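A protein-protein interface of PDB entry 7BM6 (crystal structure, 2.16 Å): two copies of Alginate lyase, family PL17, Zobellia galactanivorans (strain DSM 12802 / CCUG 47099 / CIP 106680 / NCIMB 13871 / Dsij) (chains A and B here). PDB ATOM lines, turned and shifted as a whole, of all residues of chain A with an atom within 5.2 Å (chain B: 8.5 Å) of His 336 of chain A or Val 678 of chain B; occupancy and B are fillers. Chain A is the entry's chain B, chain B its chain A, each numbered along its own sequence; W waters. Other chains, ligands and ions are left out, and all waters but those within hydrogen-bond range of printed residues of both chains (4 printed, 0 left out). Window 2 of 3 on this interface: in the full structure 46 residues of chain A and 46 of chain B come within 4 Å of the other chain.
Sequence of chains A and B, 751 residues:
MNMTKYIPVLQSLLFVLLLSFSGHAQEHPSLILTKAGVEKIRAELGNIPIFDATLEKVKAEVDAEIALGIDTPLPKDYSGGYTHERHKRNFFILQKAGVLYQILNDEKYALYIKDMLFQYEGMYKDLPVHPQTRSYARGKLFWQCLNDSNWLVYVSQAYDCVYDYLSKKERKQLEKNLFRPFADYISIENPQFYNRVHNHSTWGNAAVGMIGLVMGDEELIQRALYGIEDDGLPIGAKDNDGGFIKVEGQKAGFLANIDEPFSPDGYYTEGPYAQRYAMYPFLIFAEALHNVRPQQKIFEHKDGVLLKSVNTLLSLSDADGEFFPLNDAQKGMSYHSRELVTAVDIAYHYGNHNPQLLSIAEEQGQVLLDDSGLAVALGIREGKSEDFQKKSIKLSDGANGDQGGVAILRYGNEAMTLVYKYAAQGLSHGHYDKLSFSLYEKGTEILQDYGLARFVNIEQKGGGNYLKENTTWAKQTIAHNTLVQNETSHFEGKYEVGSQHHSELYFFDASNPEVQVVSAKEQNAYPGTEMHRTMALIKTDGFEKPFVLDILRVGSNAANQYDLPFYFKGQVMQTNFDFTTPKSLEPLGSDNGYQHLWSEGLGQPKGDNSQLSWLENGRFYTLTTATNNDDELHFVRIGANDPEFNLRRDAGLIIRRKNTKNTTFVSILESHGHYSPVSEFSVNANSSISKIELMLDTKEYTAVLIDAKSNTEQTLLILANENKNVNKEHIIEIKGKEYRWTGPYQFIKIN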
ATOM      1  N   ASP A 320      -7.721 -22.856 -15.877  1.00  0.00           N
ATOM      2  CA  ASP A 320      -6.614 -23.608 -15.276  1.00  0.00           C
ATOM      3  C   ASP A 320      -5.259 -23.129 -15.723  1.00  0.00           C
ATOM      4  O   ASP A 320      -4.274 -23.770 -15.445  1.00  0.00           O
ATOM      5  CB  ASP A 320      -6.712 -25.089 -15.701  1.00  0.00           C
ATOM      6  CG  ASP A 320      -7.976 -25.760 -15.213  1.00  0.00           C
ATOM      7  OD1 ASP A 320      -8.346 -25.527 -14.055  1.00  0.00           O
ATOM      8  OD2 ASP A 320      -8.566 -26.552 -16.001  1.00  0.00           O
ATOM      9  N   GLY A 321      -5.188 -22.048 -16.478  1.00  0.00           N
ATOM     10  CA  GLY A 321      -3.901 -21.588 -16.988  1.00  0.00           C
ATOM     11  C   GLY A 321      -3.424 -22.274 -18.252  1.00  0.00           C
ATOM     12  O   GLY A 321      -2.279 -22.016 -18.671  1.00  0.00           O
ATOM     13  N   GLY A 332      -2.678 -28.895 -22.794  1.00  0.00           N
ATOM     14  CA  GLY A 332      -1.951 -29.077 -21.545  1.00  0.00           C
ATOM     15  C   GLY A 332      -0.824 -28.086 -21.334  1.00  0.00           C
ATOM     16  O   GLY A 332      -0.449 -27.839 -20.178  1.00  0.00           O
ATOM     17  N   MET A 333      -0.275 -27.492 -22.407  1.00  0.00           N
ATOM     18  CA  MET A 333       0.700 -26.430 -22.251  1.00  0.00           C
ATOM     19  C   MET A 333       0.031 -25.254 -21.529  1.00  0.00           C
ATOM     20  O   MET A 333      -1.109 -24.878 -21.867  1.00  0.00           O
ATOM     21  CB  MET A 333       1.282 -25.967 -23.555  1.00  0.00           C
ATOM     22  CG  MET A 333       2.335 -24.842 -23.460  1.00  0.00           C
ATOM     23  SD  MET A 333       3.756 -25.102 -22.374  1.00  0.00           S
ATOM     24  CE  MET A 333       4.611 -26.452 -23.234  1.00  0.00           C
ATOM     25  N   SER A 334       0.709 -24.745 -20.519  1.00  0.00           N
ATOM     26  CA  SER A 334       0.173 -23.734 -19.639  1.00  0.00           C
ATOM     27  C   SER A 334       1.149 -22.707 -19.108  1.00  0.00           C
ATOM     28  O   SER A 334       2.316 -22.799 -19.353  1.00  0.00           O
ATOM     29  CB  SER A 334      -0.391 -24.447 -18.423  1.00  0.00           C
ATOM     30  OG  SER A 334       0.644 -24.883 -17.584  1.00  0.00           O
ATOM     31  N   TYR A 335       0.637 -21.755 -18.347  1.00  0.00           N
ATOM     32  CA  TYR A 335       1.482 -20.721 -17.782  1.00  0.00           C
ATOM     33  C   TYR A 335       2.339 -21.147 -16.622  1.00  0.00           C
ATOM     34  O   TYR A 335       2.949 -20.394 -15.962  1.00  0.00           O
ATOM     35  CB  TYR A 335       0.789 -19.411 -17.536  1.00  0.00           C
ATOM     36  CG  TYR A 335      -0.319 -19.383 -16.558  1.00  0.00           C
ATOM     37  CD1 TYR A 335      -0.156 -19.811 -15.265  1.00  0.00           C
ATOM     38  CD2 TYR A 335      -1.527 -18.844 -16.932  1.00  0.00           C
ATOM     39  CE1 TYR A 335      -1.189 -19.723 -14.370  1.00  0.00           C
ATOM     40  CE2 TYR A 335      -2.555 -18.742 -16.063  1.00  0.00           C
ATOM     41  CZ  TYR A 335      -2.401 -19.175 -14.788  1.00  0.00           C
ATOM     42  OH  TYR A 335      -3.458 -19.068 -13.954  1.00  0.00           O
ATOM     43  N   HIS A 336       2.373 -22.428 -16.442  1.00  0.00           N
ATOM     44  CA  HIS A 336       3.254 -23.005 -15.431  1.00  0.00           C
ATOM     45  C   HIS A 336       4.587 -23.430 -16.038  1.00  0.00           C
ATOM     46  O   HIS A 336       5.510 -23.830 -15.327  1.00  0.00           O
ATOM     47  CB  HIS A 336       2.580 -24.200 -14.753  1.00  0.00           C
ATOM     48  CG  HIS A 336       1.529 -23.816 -13.758  1.00  0.00           C
ATOM     49  ND1 HIS A 336       1.787 -23.698 -12.410  1.00  0.00           N
ATOM     50  CD2 HIS A 336       0.216 -23.524 -13.917  1.00  0.00           C
ATOM     51  CE1 HIS A 336       0.680 -23.349 -11.780  1.00  0.00           C
ATOM     52  NE2 HIS A 336      -0.288 -23.237 -12.671  1.00  0.00           N
ATOM     53  N   SER A 337       4.677 -23.340 -17.360  1.00  0.00           N
ATOM     54  CA  SER A 337       5.873 -23.704 -18.085  1.00  0.00           C
ATOM     55  C   SER A 337       7.051 -22.777 -17.722  1.00  0.00           C
ATOM     56  O   SER A 337       6.826 -21.642 -17.186  1.00  0.00           O
ATOM     57  CB  SER A 337       5.586 -23.657 -19.589  1.00  0.00           C
ATOM     58  OG  SER A 337       5.569 -22.333 -20.074  1.00  0.00           O
ATOM     59  N   ARG A 338       8.278 -23.256 -17.989  1.00  0.00           N
ATOM     60  CA  ARG A 338       9.515 -22.533 -17.628  1.00  0.00           C
ATOM     61  C   ARG A 338       9.550 -21.194 -18.390  1.00  0.00           C
ATOM     62  O   ARG A 338       9.999 -20.145 -17.850  1.00  0.00           O
ATOM     63  CB  ARG A 338      10.757 -23.388 -17.904  1.00  0.00           C
ATOM     64  CG  ARG A 338      10.962 -23.716 -19.395  1.00  0.00           C
ATOM     65  CD  ARG A 338      12.119 -24.671 -19.625  1.00  0.00           C
ATOM     66  NE  ARG A 338      11.793 -26.030 -19.252  1.00  0.00           N
ATOM     67  CZ  ARG A 338      11.316 -26.951 -20.090  1.00  0.00           C
ATOM     68  NH1 ARG A 338      11.054 -26.685 -21.365  1.00  0.00           N
ATOM     69  NH2 ARG A 338      11.124 -28.187 -19.672  1.00  0.00           N
ATOM     70  N   LEU A 340       6.984 -19.285 -19.109  1.00  0.00           N
ATOM     71  CA  LEU A 340       6.112 -18.289 -18.420  1.00  0.00           C
ATOM     72  C   LEU A 340       6.612 -17.880 -17.032  1.00  0.00           C
ATOM     73  O   LEU A 340       6.338 -16.769 -16.564  1.00  0.00           O
ATOM     74  CB  LEU A 340       4.683 -18.743 -18.355  1.00  0.00           C
ATOM     75  CG  LEU A 340       3.806 -18.436 -19.569  1.00  0.00           C
ATOM     76  CD1 LEU A 340       3.575 -16.940 -19.786  1.00  0.00           C
ATOM     77  CD2 LEU A 340       4.341 -19.074 -20.829  1.00  0.00           C
ATOM     78  N   VAL A 341       7.405 -18.726 -16.410  1.00  0.00           N
ATOM     79  CA  VAL A 341       8.070 -18.334 -15.164  1.00  0.00           C
ATOM     80  C   VAL A 341       9.007 -17.216 -15.474  1.00  0.00           C
ATOM     81  O   VAL A 341       9.015 -16.172 -14.770  1.00  0.00           O
ATOM     82  CB  VAL A 341       8.828 -19.521 -14.482  1.00  0.00           C
ATOM     83  CG1 VAL A 341       9.639 -19.101 -13.268  1.00  0.00           C
ATOM     84  CG2 VAL A 341       7.842 -20.538 -14.011  1.00  0.00           C
ATOM     85  N   GLU A 363       0.921 -18.801  -8.037  1.00  0.00           N
ATOM     86  CA  GLU A 363       0.409 -20.053  -8.607  1.00  0.00           C
ATOM     87  C   GLU A 363       1.522 -20.915  -9.177  1.00  0.00           C
ATOM     88  O   GLU A 363       1.440 -22.132  -9.081  1.00  0.00           O
ATOM     89  CB  GLU A 363      -0.606 -19.801  -9.731  1.00  0.00           C
ATOM     90  CG  GLU A 363      -1.908 -19.201  -9.234  1.00  0.00           C
ATOM     91  CD  GLU A 363      -2.941 -18.888 -10.336  1.00  0.00           C
ATOM     92  OE1 GLU A 363      -2.908 -19.509 -11.437  1.00  0.00           O
ATOM     93  OE2 GLU A 363      -3.807 -18.008 -10.094  1.00  0.00           O
ATOM     94  N   GLN A 364       2.489 -20.306  -9.873  1.00  0.00           N
ATOM     95  CA  GLN A 364       3.633 -21.047 -10.396  1.00  0.00           C
ATOM     96  C   GLN A 364       4.404 -21.724  -9.234  1.00  0.00           C
ATOM     97  O   GLN A 364       4.847 -22.836  -9.345  1.00  0.00           O
ATOM     98  CB  GLN A 364       4.551 -20.136 -11.216  1.00  0.00           C
ATOM     99  CG  GLN A 364       3.931 -19.656 -12.528  1.00  0.00           C
ATOM    100  CD  GLN A 364       4.698 -18.511 -13.197  1.00  0.00           C
ATOM    101  OE1 GLN A 364       5.365 -17.706 -12.528  1.00  0.00           O
ATOM    102  NE2 GLN A 364       4.553 -18.390 -14.511  1.00  0.00           N
ATOM    103  N   GLN A 366       7.338 -20.944  -8.137  1.00  0.00           N
ATOM    104  CA  GLN A 366       8.789 -20.819  -8.269  1.00  0.00           C
ATOM    105  C   GLN A 366       9.090 -19.505  -8.942  1.00  0.00           C
ATOM    106  O   GLN A 366       8.178 -18.859  -9.492  1.00  0.00           O
ATOM    107  CB  GLN A 366       9.379 -22.006  -9.079  1.00  0.00           C
ATOM    108  CG  GLN A 366       8.774 -22.140 -10.476  1.00  0.00           C
ATOM    109  CD  GLN A 366       9.174 -23.430 -11.169  1.00  0.00           C
ATOM    110  OE1 GLN A 366      10.230 -23.985 -10.894  1.00  0.00           O
ATOM    111  NE2 GLN A 366       8.333 -23.918 -12.043  1.00  0.00           N
ATOM    112  N   TYR B 675       5.033 -38.514 -18.644  1.00  0.00           N
ATOM    113  CA  TYR B 675       4.972 -37.484 -19.679  1.00  0.00           C
ATOM    114  C   TYR B 675       4.230 -36.304 -19.094  1.00  0.00           C
ATOM    115  O   TYR B 675       3.238 -36.486 -18.421  1.00  0.00           O
ATOM    116  CB  TYR B 675       4.284 -37.932 -20.970  1.00  0.00           C
ATOM    117  CG  TYR B 675       4.363 -36.860 -22.004  1.00  0.00           C
ATOM    118  CD1 TYR B 675       5.578 -36.606 -22.659  1.00  0.00           C
ATOM    119  CD2 TYR B 675       3.284 -35.984 -22.251  1.00  0.00           C
ATOM    120  CE1 TYR B 675       5.704 -35.569 -23.557  1.00  0.00           C
ATOM    121  CE2 TYR B 675       3.399 -34.940 -23.142  1.00  0.00           C
ATOM    122  CZ  TYR B 675       4.619 -34.739 -23.812  1.00  0.00           C
ATOM    123  OH  TYR B 675       4.780 -33.704 -24.733  1.00  0.00           O
ATOM    124  N   SER B 676       4.749 -35.105 -19.329  1.00  0.00           N
ATOM    125  CA  SER B 676       4.083 -33.875 -18.922  1.00  0.00           C
ATOM    126  C   SER B 676       3.957 -32.964 -20.132  1.00  0.00           C
ATOM    127  O   SER B 676       4.955 -32.662 -20.739  1.00  0.00           O
ATOM    128  CB  SER B 676       4.914 -33.136 -17.864  1.00  0.00           C
ATOM    129  OG  SER B 676       4.419 -31.816 -17.763  1.00  0.00           O
ATOM    130  N   PRO B 677       2.738 -32.492 -20.457  1.00  0.00           N
ATOM    131  CA  PRO B 677       2.667 -31.468 -21.533  1.00  0.00           C
ATOM    132  C   PRO B 677       3.092 -30.025 -21.092  1.00  0.00           C
ATOM    133  O   PRO B 677       2.927 -29.077 -21.859  1.00  0.00           O
ATOM    134  CB  PRO B 677       1.155 -31.493 -21.925  1.00  0.00           C
ATOM    135  CG  PRO B 677       0.441 -31.874 -20.621  1.00  0.00           C
ATOM    136  CD  PRO B 677       1.395 -32.816 -19.887  1.00  0.00           C
ATOM    137  N   VAL B 678       3.518 -29.842 -19.837  1.00  0.00           N
ATOM    138  CA  VAL B 678       4.011 -28.556 -19.341  1.00  0.00           C
ATOM    139  C   VAL B 678       5.531 -28.480 -19.608  1.00  0.00           C
ATOM    140  O   VAL B 678       6.043 -27.528 -20.193  1.00  0.00           O
ATOM    141  CB  VAL B 678       3.696 -28.397 -17.837  1.00  0.00           C
ATOM    142  CG1 VAL B 678       4.257 -27.066 -17.300  1.00  0.00           C
ATOM    143  CG2 VAL B 678       2.183 -28.454 -17.574  1.00  0.00           C
ATOM    144  N   SER B 679       6.252 -29.509 -19.192  1.00  0.00           N
ATOM    145  CA  SER B 679       7.679 -29.558 -19.421  1.00  0.00           C
ATOM    146  C   SER B 679       8.009 -30.123 -20.825  1.00  0.00           C
ATOM    147  O   SER B 679       9.126 -29.933 -21.299  1.00  0.00           O
ATOM    148  CB  SER B 679       8.339 -30.375 -18.322  1.00  0.00           C
ATOM    149  OG  SER B 679       8.083 -31.747 -18.559  1.00  0.00           O
ATOM    150  N   GLU B 680       7.058 -30.830 -21.438  1.00  0.00           N
ATOM    151  CA  GLU B 680       7.268 -31.627 -22.644  1.00  0.00           C
ATOM    152  C   GLU B 680       8.406 -32.680 -22.558  1.00  0.00           C
ATOM    153  O   GLU B 680       8.988 -33.038 -23.588  1.00  0.00           O
ATOM    154  CB  GLU B 680       7.421 -30.705 -23.855  1.00  0.00           C
ATOM    155  CG  GLU B 680       6.194 -29.810 -24.040  1.00  0.00           C
ATOM    156  CD  GLU B 680       6.224 -28.974 -25.321  1.00  0.00           C
ATOM    157  OE1 GLU B 680       7.322 -28.511 -25.720  1.00  0.00           O
ATOM    158  OE2 GLU B 680       5.136 -28.773 -25.924  1.00  0.00           O
ATOM    159  N   PHE B 681       8.660 -33.208 -21.358  1.00  0.00           N
ATOM    160  CA  PHE B 681       9.614 -34.319 -21.121  1.00  0.00           C
ATOM    161  C   PHE B 681       8.914 -35.671 -21.049  1.00  0.00           C
ATOM    162  O   PHE B 681       7.982 -35.861 -20.273  1.00  0.00           O
ATOM    163  CB  PHE B 681      10.421 -34.097 -19.813  1.00  0.00           C
ATOM    164  CG  PHE B 681      11.682 -33.296 -19.999  1.00  0.00           C
ATOM    165  CD1 PHE B 681      12.858 -33.908 -20.468  1.00  0.00           C
ATOM    166  CD2 PHE B 681      11.724 -31.929 -19.702  1.00  0.00           C
ATOM    167  CE1 PHE B 681      14.045 -33.159 -20.640  1.00  0.00           C
ATOM    168  CE2 PHE B 681      12.894 -31.182 -19.869  1.00  0.00           C
ATOM    169  CZ  PHE B 681      14.057 -31.794 -20.336  1.00  0.00           C
HETATM  170  O   HOH W   1       8.962 -27.024 -24.105  1.00  0.00           O
HETATM  171  O   HOH W   2       7.899 -25.654 -21.859  1.00  0.00           O
HETATM  172  O   HOH W   3      11.060 -29.253 -23.371  1.00  0.00           O
HETATM  173  O   HOH W   4       8.189 -25.955 -18.987  1.00  0.00           O
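The backbone carbonyl oxygen (O) of Ser 679 of chain B is in hydrogen-bond range of the guanidinium group (NH2) of Arg 338 of chain A.
The backbone NH of Val 678 of chain B is in hydrogen-bond range of the side-chain hydroxyl of Ser 676 of chain B. The backbone NH of Ser 679 of chain B sits at hydrogen-bond distance from the side-chain hydroxyl of Ser 676 of chain B, at 3.3 Å. N of Ser 676 of chain B is in hydrogen-bond range of O of Phe 681 of chain B (3.5 Å). N of Phe 681 of chain B sits close to OG of Ser 679 of chain B, 3.2 Å away. The backbone carbonyl oxygen of Ser 334 of chain A lies within hydrogen-bond range of the side-chain hydroxyl of Ser 337 of chain A, at 3.4 Å. The side-chain hydroxyl (OG) of Ser 337 of chain A lies within hydrogen-bond range of the backbone NH (N) of Leu 340 of chain A (3.5 Å).
Among the printed residues, merely in contact across the chains: Gly 332 of chain A with Pro 677 of chain B (3.8 Å), Gly 332 of chain A with Val 678 of chain B (3.8 Å), Met 333 of chain A with Pro 677 of chain B (3.4 Å), Met 333 of chain A with Val 678 of chain B (3.5 Å), Met 333 of chain A with Glu 680 of chain B (3.6 Å), Ser 334 of chain A with Val 678 of chain B (3.9 Å), His 336 of chain A with Val 678 of chain B (3.9 Å), Ser 337 of chain A with Val 678 of chain B (3.8 Å) and Arg 338 of chain A with Phe 681 of chain B (3.5 Å).
Of the printed residues of chain B, Gly 332 of chain A touches Pro 677 (3.8 Å) and Val 678 (3.8 Å). Of the printed residues of chain B, Met 333 of chain A touches Pro 677, Val 678 and Glu 680. Of chain B, only Val 678 comes within 4 Å of His 336 of chain A. Printed residues of chain A within 4 Å of Val 678 of chain B: Gly 332 (3.8 Å), Met 333 (3.5 Å), Ser 334 (3.9 Å), His 336 (3.9 Å) and Ser 337 (3.8 Å). Printed residues of chain A within 4 Å of Ser 679 of chain B: Arg 338. Of the printed residues of chain A, Glu 680 of chain B touches Met 333. Of the printed residues of chain A, Phe 681 of chain B touches Arg 338 (3.5 Å). The nearest residue of chain A that does not touch Val 678 of chain B is Arg 338 of chain A (5.1 Å).
Printed residues of chain B that touch a printed residue of chain A: Pro 677, Val 678, Ser 679, Glu 680 and Phe 681. Hydrophobic or aromatic side chains of chain B within 4 Å of the printed part of chain A: Pro 677, Val 678 and Phe 681. Among the printed residues, 10 pairs touch across the chains. Among the printed residues, no Asp or Glu carboxylate lies within 4 Å of a Lys or Arg side-chain nitrogen of the other chain.
No position is printed for both chains. Of the 10 pairs that touch across the chains among the printed residues, none has its exchanged pair printed and touching as well.
Water W1 bridges OE1 of Glu 680 of chain B and NH1 of Arg 338 of chain A. Water W4 lies within hydrogen-bond range of the backbone NH of Arg 338 of chain A (2.9 Å) and the backbone carbonyl oxygen of Val 678 of chain B (2.9 Å). Water W3 bridges the backbone carbonyl oxygen of Ser 679 of chain B (2.9 Å) and the guanidinium group of Arg 338 of chain A (3.3 Å). Water W2 lies within hydrogen-bond range of O of Val 678 of chain B and NH1 of Arg 338 of chain A.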
